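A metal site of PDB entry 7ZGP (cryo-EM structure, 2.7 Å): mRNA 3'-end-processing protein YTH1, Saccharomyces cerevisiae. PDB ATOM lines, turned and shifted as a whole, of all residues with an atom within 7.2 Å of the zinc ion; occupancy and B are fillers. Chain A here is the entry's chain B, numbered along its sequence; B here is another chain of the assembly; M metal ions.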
ATOM      1  N   ILE A  60      21.462 -37.023 -21.501  1.00  0.00           N
ATOM      2  CA  ILE A  60      21.333 -35.826 -20.686  1.00  0.00           C
ATOM      3  C   ILE A  60      22.557 -35.601 -19.805  1.00  0.00           C
ATOM      4  O   ILE A  60      22.875 -34.459 -19.464  1.00  0.00           O
ATOM      5  CB  ILE A  60      20.039 -35.916 -19.842  1.00  0.00           C
ATOM      6  CG1 ILE A  60      19.831 -34.642 -19.002  1.00  0.00           C
ATOM      7  CG2 ILE A  60      20.048 -37.142 -18.953  1.00  0.00           C
ATOM      8  CD1 ILE A  60      19.513 -33.420 -19.816  1.00  0.00           C
ATOM      9  N   ASN A  63      26.064 -33.735 -21.191  1.00  0.00           N
ATOM     10  CA  ASN A  63      26.104 -32.296 -21.387  1.00  0.00           C
ATOM     11  C   ASN A  63      27.146 -31.666 -20.474  1.00  0.00           C
ATOM     12  O   ASN A  63      27.486 -32.192 -19.416  1.00  0.00           O
ATOM     13  CB  ASN A  63      24.727 -31.690 -21.135  1.00  0.00           C
ATOM     14  CG  ASN A  63      23.663 -32.251 -22.056  1.00  0.00           C
ATOM     15  OD1 ASN A  63      23.966 -32.700 -23.164  1.00  0.00           O
ATOM     16  ND2 ASN A  63      22.419 -32.249 -21.603  1.00  0.00           N
ATOM     17  N   VAL A  66      25.678 -27.379 -16.182  1.00  0.00           N
ATOM     18  CA  VAL A  66      24.493 -27.702 -15.399  1.00  0.00           C
ATOM     19  C   VAL A  66      23.348 -26.789 -15.802  1.00  0.00           C
ATOM     20  O   VAL A  66      23.516 -25.568 -15.960  1.00  0.00           O
ATOM     21  CB  VAL A  66      24.800 -27.583 -13.900  1.00  0.00           C
ATOM     22  CG1 VAL A  66      23.566 -27.881 -13.071  1.00  0.00           C
ATOM     23  CG2 VAL A  66      25.942 -28.513 -13.529  1.00  0.00           C
ATOM     24  N   CYS A  67      22.159 -27.365 -15.977  1.00  0.00           N
ATOM     25  CA  CYS A  67      20.987 -26.594 -16.345  1.00  0.00           C
ATOM     26  C   CYS A  67      20.557 -25.700 -15.187  1.00  0.00           C
ATOM     27  O   CYS A  67      20.275 -26.185 -14.086  1.00  0.00           O
ATOM     28  CB  CYS A  67      19.845 -27.531 -16.745  1.00  0.00           C
ATOM     29  SG  CYS A  67      18.288 -26.708 -17.118  1.00  0.00           S
ATOM     30  N   ARG A  68      20.490 -24.397 -15.444  1.00  0.00           N
ATOM     31  CA  ARG A  68      20.106 -23.464 -14.392  1.00  0.00           C
ATOM     32  C   ARG A  68      18.646 -23.636 -13.992  1.00  0.00           C
ATOM     33  O   ARG A  68      18.298 -23.388 -12.832  1.00  0.00           O
ATOM     34  CB  ARG A  68      20.375 -22.023 -14.847  1.00  0.00           C
ATOM     35  CG  ARG A  68      19.386 -21.473 -15.860  1.00  0.00           C
ATOM     36  CD  ARG A  68      19.657 -20.012 -16.167  1.00  0.00           C
ATOM     37  NE  ARG A  68      20.744 -19.851 -17.125  1.00  0.00           N
ATOM     38  CZ  ARG A  68      21.974 -19.443 -16.814  1.00  0.00           C
ATOM     39  NH1 ARG A  68      22.303 -19.149 -15.569  1.00  0.00           N
ATOM     40  NH2 ARG A  68      22.882 -19.329 -17.770  1.00  0.00           N
ATOM     41  N   HIS A  69      17.789 -24.043 -14.922  1.00  0.00           N
ATOM     42  CA  HIS A  69      16.380 -24.264 -14.594  1.00  0.00           C
ATOM     43  C   HIS A  69      16.165 -25.571 -13.850  1.00  0.00           C
ATOM     44  O   HIS A  69      15.228 -25.673 -13.052  1.00  0.00           O
ATOM     45  CB  HIS A  69      15.544 -24.234 -15.879  1.00  0.00           C
ATOM     46  CG  HIS A  69      15.819 -23.060 -16.753  1.00  0.00           C
ATOM     47  ND1 HIS A  69      16.767 -23.079 -17.761  1.00  0.00           N
ATOM     48  CD2 HIS A  69      15.283 -21.811 -16.774  1.00  0.00           C
ATOM     49  CE1 HIS A  69      16.789 -21.902 -18.355  1.00  0.00           C
ATOM     50  NE2 HIS A  69      15.904 -21.116 -17.779  1.00  0.00           N
ATOM     51  N   TRP A  70      17.009 -26.562 -14.092  1.00  0.00           N
ATOM     52  CA  TRP A  70      16.915 -27.818 -13.353  1.00  0.00           C
ATOM     53  C   TRP A  70      17.233 -27.617 -11.874  1.00  0.00           C
ATOM     54  O   TRP A  70      16.611 -28.245 -11.007  1.00  0.00           O
ATOM     55  CB  TRP A  70      17.845 -28.863 -13.968  1.00  0.00           C
ATOM     56  CG  TRP A  70      17.849 -30.163 -13.231  1.00  0.00           C
ATOM     57  CD1 TRP A  70      16.910 -31.138 -13.274  1.00  0.00           C
ATOM     58  CD2 TRP A  70      18.867 -30.638 -12.340  1.00  0.00           C
ATOM     59  NE1 TRP A  70      17.260 -32.187 -12.468  1.00  0.00           N
ATOM     60  CE2 TRP A  70      18.467 -31.899 -11.879  1.00  0.00           C
ATOM     61  CE3 TRP A  70      20.081 -30.116 -11.885  1.00  0.00           C
ATOM     62  CZ2 TRP A  70      19.232 -32.652 -10.991  1.00  0.00           C
ATOM     63  CZ3 TRP A  70      20.837 -30.857 -11.010  1.00  0.00           C
ATOM     64  CH2 TRP A  70      20.409 -32.112 -10.571  1.00  0.00           C
ATOM     65  N   LEU A  71      18.201 -26.739 -11.567  1.00  0.00           N
ATOM     66  CA  LEU A  71      18.563 -26.502 -10.179  1.00  0.00           C
ATOM     67  C   LEU A  71      17.400 -25.888  -9.401  1.00  0.00           C
ATOM     68  O   LEU A  71      17.275 -26.124  -8.191  1.00  0.00           O
ATOM     69  CB  LEU A  71      19.786 -25.581 -10.109  1.00  0.00           C
ATOM     70  CG  LEU A  71      21.068 -26.141 -10.726  1.00  0.00           C
ATOM     71  CD1 LEU A  71      22.109 -25.053 -10.850  1.00  0.00           C
ATOM     72  CD2 LEU A  71      21.597 -27.298  -9.887  1.00  0.00           C
ATOM     73  N   LEU A  74      12.697 -26.283 -12.404  1.00  0.00           N
ATOM     74  CA  LEU A  74      11.827 -25.631 -13.382  1.00  0.00           C
ATOM     75  C   LEU A  74      12.370 -25.843 -14.791  1.00  0.00           C
ATOM     76  O   LEU A  74      12.304 -24.938 -15.630  1.00  0.00           O
ATOM     77  CB  LEU A  74      11.696 -24.138 -13.080  1.00  0.00           C
ATOM     78  CG  LEU A  74      10.967 -23.775 -11.783  1.00  0.00           C
ATOM     79  CD1 LEU A  74      11.145 -22.299 -11.480  1.00  0.00           C
ATOM     80  CD2 LEU A  74       9.500 -24.137 -11.875  1.00  0.00           C
ATOM     81  N   CYS A  75      12.882 -27.033 -15.077  1.00  0.00           N
ATOM     82  CA  CYS A  75      13.370 -27.369 -16.412  1.00  0.00           C
ATOM     83  C   CYS A  75      12.222 -27.927 -17.223  1.00  0.00           C
ATOM     84  O   CYS A  75      11.660 -28.974 -16.874  1.00  0.00           O
ATOM     85  CB  CYS A  75      14.523 -28.367 -16.342  1.00  0.00           C
ATOM     86  SG  CYS A  75      15.208 -28.811 -17.946  1.00  0.00           S
ATOM     87  N   LYS A  76      11.876 -27.253 -18.318  1.00  0.00           N
ATOM     88  CA  LYS A  76      10.768 -27.669 -19.157  1.00  0.00           C
ATOM     89  C   LYS A  76      11.144 -28.734 -20.177  1.00  0.00           C
ATOM     90  O   LYS A  76      10.259 -29.307 -20.809  1.00  0.00           O
ATOM     91  CB  LYS A  76      10.164 -26.461 -19.889  1.00  0.00           C
ATOM     92  CG  LYS A  76       9.456 -25.478 -18.969  1.00  0.00           C
ATOM     93  CD  LYS A  76       9.029 -24.241 -19.736  1.00  0.00           C
ATOM     94  CE  LYS A  76       8.774 -23.076 -18.797  1.00  0.00           C
ATOM     95  NZ  LYS A  76       7.636 -23.352 -17.872  1.00  0.00           N
ATOM     96  N   LYS A  77      12.436 -29.006 -20.348  1.00  0.00           N
ATOM     97  CA  LYS A  77      12.874 -29.961 -21.365  1.00  0.00           C
ATOM     98  C   LYS A  77      13.109 -31.366 -20.822  1.00  0.00           C
ATOM     99  O   LYS A  77      13.109 -32.315 -21.612  1.00  0.00           O
ATOM    100  CB  LYS A  77      14.162 -29.455 -22.021  1.00  0.00           C
ATOM    101  CG  LYS A  77      14.000 -28.116 -22.716  1.00  0.00           C
ATOM    102  CD  LYS A  77      15.321 -27.612 -23.269  1.00  0.00           C
ATOM    103  CE  LYS A  77      15.186 -26.207 -23.821  1.00  0.00           C
ATOM    104  NZ  LYS A  77      16.509 -25.599 -24.093  1.00  0.00           N
ATOM    105  N   ASN A  78      13.289 -31.507 -19.512  1.00  0.00           N
ATOM    106  CA  ASN A  78      13.445 -32.817 -18.847  1.00  0.00           C
ATOM    107  C   ASN A  78      14.659 -33.513 -19.458  1.00  0.00           C
ATOM    108  O   ASN A  78      15.721 -32.872 -19.588  1.00  0.00           O
ATOM    109  CB  ASN A  78      12.131 -33.575 -18.942  1.00  0.00           C
ATOM    110  CG  ASN A  78      10.956 -32.777 -18.431  1.00  0.00           C
ATOM    111  OD1 ASN A  78      10.912 -32.381 -17.260  1.00  0.00           O
ATOM    112  ND2 ASN A  78       9.982 -32.530 -19.300  1.00  0.00           N
ATOM    113  N   ASP A  79      14.574 -34.792 -19.819  1.00  0.00           N
ATOM    114  CA  ASP A  79      15.723 -35.515 -20.345  1.00  0.00           C
ATOM    115  C   ASP A  79      16.156 -35.042 -21.728  1.00  0.00           C
ATOM    116  O   ASP A  79      17.256 -35.397 -22.165  1.00  0.00           O
ATOM    117  CB  ASP A  79      15.411 -37.016 -20.401  1.00  0.00           C
ATOM    118  CG  ASP A  79      14.971 -37.561 -19.054  1.00  0.00           C
ATOM    119  OD1 ASP A  79      15.813 -37.636 -18.138  1.00  0.00           O
ATOM    120  OD2 ASP A  79      13.782 -37.919 -18.927  1.00  0.00           O
ATOM    121  N   GLN A  80      15.335 -34.252 -22.410  1.00  0.00           N
ATOM    122  CA  GLN A  80      15.702 -33.716 -23.713  1.00  0.00           C
ATOM    123  C   GLN A  80      16.496 -32.421 -23.625  1.00  0.00           C
ATOM    124  O   GLN A  80      16.862 -31.862 -24.664  1.00  0.00           O
ATOM    125  CB  GLN A  80      14.437 -33.479 -24.558  1.00  0.00           C
ATOM    126  CG  GLN A  80      13.333 -34.485 -24.320  1.00  0.00           C
ATOM    127  CD  GLN A  80      13.783 -35.920 -24.492  1.00  0.00           C
ATOM    128  OE1 GLN A  80      14.367 -36.274 -25.514  1.00  0.00           O
ATOM    129  NE2 GLN A  80      13.524 -36.758 -23.493  1.00  0.00           N
ATOM    130  N   CYS A  81      16.785 -31.943 -22.419  1.00  0.00           N
ATOM    131  CA  CYS A  81      17.541 -30.718 -22.245  1.00  0.00           C
ATOM    132  C   CYS A  81      18.956 -30.879 -22.777  1.00  0.00           C
ATOM    133  O   CYS A  81      19.553 -31.956 -22.704  1.00  0.00           O
ATOM    134  CB  CYS A  81      17.568 -30.314 -20.766  1.00  0.00           C
ATOM    135  SG  CYS A  81      18.142 -28.641 -20.437  1.00  0.00           S
ATOM    136  N   GLU A  82      19.496 -29.789 -23.320  1.00  0.00           N
ATOM    137  CA  GLU A  82      20.863 -29.773 -23.828  1.00  0.00           C
ATOM    138  C   GLU A  82      21.885 -29.412 -22.760  1.00  0.00           C
ATOM    139  O   GLU A  82      23.067 -29.327 -23.063  1.00  0.00           O
ATOM    140  CB  GLU A  82      20.987 -28.804 -25.011  1.00  0.00           C
ATOM    141  CG  GLU A  82      19.738 -28.671 -25.860  1.00  0.00           C
ATOM    142  CD  GLU A  82      18.797 -27.602 -25.355  1.00  0.00           C
ATOM    143  OE1 GLU A  82      17.572 -27.756 -25.523  1.00  0.00           O
ATOM    144  OE2 GLU A  82      19.285 -26.592 -24.792  1.00  0.00           O
ATOM    145  N   TYR A  83      21.438 -29.182 -21.529  1.00  0.00           N
ATOM    146  CA  TYR A  83      22.312 -28.853 -20.419  1.00  0.00           C
ATOM    147  C   TYR A  83      22.264 -29.958 -19.365  1.00  0.00           C
ATOM    148  O   TYR A  83      21.317 -30.745 -19.307  1.00  0.00           O
ATOM    149  CB  TYR A  83      21.939 -27.510 -19.806  1.00  0.00           C
ATOM    150  CG  TYR A  83      22.372 -26.334 -20.649  1.00  0.00           C
ATOM    151  CD1 TYR A  83      21.660 -25.946 -21.770  1.00  0.00           C
ATOM    152  CD2 TYR A  83      23.515 -25.615 -20.327  1.00  0.00           C
ATOM    153  CE1 TYR A  83      22.071 -24.880 -22.550  1.00  0.00           C
ATOM    154  CE2 TYR A  83      23.932 -24.546 -21.091  1.00  0.00           C
ATOM    155  CZ  TYR A  83      23.202 -24.186 -22.197  1.00  0.00           C
ATOM    156  OH  TYR A  83      23.613 -23.121 -22.977  1.00  0.00           O
ATOM    157  N   LEU A  84      23.301 -30.007 -18.549  1.00  0.00           N
ATOM    158  CA  LEU A  84      23.484 -31.117 -17.620  1.00  0.00           C
ATOM    159  C   LEU A  84      22.440 -31.067 -16.511  1.00  0.00           C
ATOM    160  O   LEU A  84      22.250 -30.029 -15.859  1.00  0.00           O
ATOM    161  CB  LEU A  84      24.884 -31.078 -17.024  1.00  0.00           C
ATOM    162  CG  LEU A  84      25.219 -32.188 -16.029  1.00  0.00           C
ATOM    163  CD1 LEU A  84      25.055 -33.544 -16.683  1.00  0.00           C
ATOM    164  CD2 LEU A  84      26.627 -32.022 -15.502  1.00  0.00           C
ATOM    165  N   HIS A  85      21.760 -32.193 -16.285  1.00  0.00           N
ATOM    166  CA  HIS A  85      20.810 -32.357 -15.190  1.00  0.00           C
ATOM    167  C   HIS A  85      21.420 -33.121 -14.025  1.00  0.00           C
ATOM    168  O   HIS A  85      20.748 -33.909 -13.366  1.00  0.00           O
ATOM    169  CB  HIS A  85      19.539 -33.031 -15.677  1.00  0.00           C
ATOM    170  CG  HIS A  85      18.557 -32.088 -16.296  1.00  0.00           C
ATOM    171  ND1 HIS A  85      17.217 -32.374 -16.402  1.00  0.00           N
ATOM    172  CD2 HIS A  85      18.719 -30.852 -16.834  1.00  0.00           C
ATOM    173  CE1 HIS A  85      16.590 -31.358 -16.979  1.00  0.00           C
ATOM    174  NE2 HIS A  85      17.481 -30.428 -17.251  1.00  0.00           N
ATOM    175  P     A B  21      23.176 -20.636 -26.273  1.00  0.00           P
ATOM    176  OP1   A B  21      22.923 -19.523 -27.213  1.00  0.00           O
ATOM    177  OP2   A B  21      23.834 -20.365 -24.970  1.00  0.00           O
ATOM    178  O5'   A B  21      21.788 -21.367 -25.999  1.00  0.00           O
ATOM    179  C5'   A B  21      20.634 -20.604 -25.667  1.00  0.00           C
ATOM    180  C4'   A B  21      19.549 -21.469 -25.077  1.00  0.00           C
ATOM    181  O4'   A B  21      20.107 -22.264 -23.985  1.00  0.00           O
ATOM    182  C3'   A B  21      18.378 -20.700 -24.470  1.00  0.00           C
ATOM    183  O3'   A B  21      17.192 -21.467 -24.603  1.00  0.00           O
ATOM    184  C2'   A B  21      18.762 -20.612 -22.995  1.00  0.00           C
ATOM    185  O2'   A B  21      17.673 -20.426 -22.115  1.00  0.00           O
ATOM    186  C1'   A B  21      19.445 -21.962 -22.783  1.00  0.00           C
ATOM    187  N9    A B  21      20.432 -21.965 -21.708  1.00  0.00           N
ATOM    188  C8    A B  21      21.590 -21.227 -21.634  1.00  0.00           C
ATOM    189  N7    A B  21      22.288 -21.444 -20.552  1.00  0.00           N
ATOM    190  C5    A B  21      21.535 -22.378 -19.854  1.00  0.00           C
ATOM    191  C6    A B  21      21.726 -23.013 -18.623  1.00  0.00           C
ATOM    192  N6    A B  21      22.790 -22.803 -17.834  1.00  0.00           N
ATOM    193  N1    A B  21      20.789 -23.898 -18.223  1.00  0.00           N
ATOM    194  C2    A B  21      19.734 -24.118 -19.013  1.00  0.00           C
ATOM    195  N3    A B  21      19.440 -23.581 -20.189  1.00  0.00           N
ATOM    196  C4    A B  21      20.398 -22.711 -20.556  1.00  0.00           C
ATOM    197  P     A B  22      15.893 -20.843 -25.316  1.00  0.00           P
ATOM    198  OP1   A B  22      15.065 -21.987 -25.738  1.00  0.00           O
ATOM    199  OP2   A B  22      16.337 -19.845 -26.316  1.00  0.00           O
ATOM    200  O5'   A B  22      15.149 -20.081 -24.131  1.00  0.00           O
ATOM    201  C5'   A B  22      14.038 -19.226 -24.392  1.00  0.00           C
ATOM    202  C4'   A B  22      13.312 -18.877 -23.112  1.00  0.00           C
ATOM    203  O4'   A B  22      12.960 -20.110 -22.434  1.00  0.00           O
ATOM    204  C3'   A B  22      14.134 -18.066 -22.113  1.00  0.00           C
ATOM    205  O3'   A B  22      13.278 -17.206 -21.370  1.00  0.00           O
ATOM    206  C2'   A B  22      14.712 -19.146 -21.198  1.00  0.00           C
ATOM    207  O2'   A B  22      15.046 -18.696 -19.894  1.00  0.00           O
ATOM    208  C1'   A B  22      13.583 -20.178 -21.162  1.00  0.00           C
ATOM    209  N9    A B  22      14.069 -21.547 -20.987  1.00  0.00           N
ATOM    210  C8    A B  22      15.104 -22.141 -21.668  1.00  0.00           C
ATOM    211  N7    A B  22      15.321 -23.388 -21.319  1.00  0.00           N
ATOM    212  C5    A B  22      14.372 -23.625 -20.346  1.00  0.00           C
ATOM    213  C6    A B  22      14.077 -24.764 -19.582  1.00  0.00           C
ATOM    214  N6    A B  22      14.753 -25.908 -19.684  1.00  0.00           N
ATOM    215  N1    A B  22      13.067 -24.681 -18.687  1.00  0.00           N
ATOM    216  C2    A B  22      12.394 -23.523 -18.590  1.00  0.00           C
ATOM    217  N3    A B  22      12.574 -22.390 -19.262  1.00  0.00           N
ATOM    218  C4    A B  22      13.582 -22.509 -20.127  1.00  0.00           C
HETATM  219 ZN    ZN M   1      17.502 -28.595 -18.215  1.00  0.00          ZN
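N of Cys 75 is in hydrogen-bond range of O of His 69 (3.4 Å). The backbone NH (N) of Cys 67 sits at hydrogen-bond distance from the backbone carbonyl oxygen (O) of Leu 84, 2.7 Å away. The side-chain sulfur of Cys 75 sits close to N6 of A 22 of chain B, at 3.4 Å. N of Asn 78 sits close to SG of Cys 75, 3.7 Å away. SG of Cys 81 lies close to N of Tyr 83 (3.5 Å). The backbone carbonyl oxygen of Cys 81 is in hydrogen-bond range of the side-chain amide nitrogen of Asn 63. The side-chain sulfur (SG) of Cys 75 lies close to the backbone NH (N) of Lys 77 (3.7 Å). SG of Cys 67 lies close to N of His 69 (3.5 Å).
Within 4 Å of the zinc ion: Cys 67, Cys 75, Cys 81 and His 85.
The zinc ion is bound by a ring nitrogen (NE2) of His 85 (2.1 Å), the side-chain sulfur of Cys 81 (2.3 Å), the side-chain sulfur of Cys 67 (2.3 Å) and the side-chain sulfur of Cys 75 (2.3 Å). The zinc ion has four donor atoms within binding distance.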
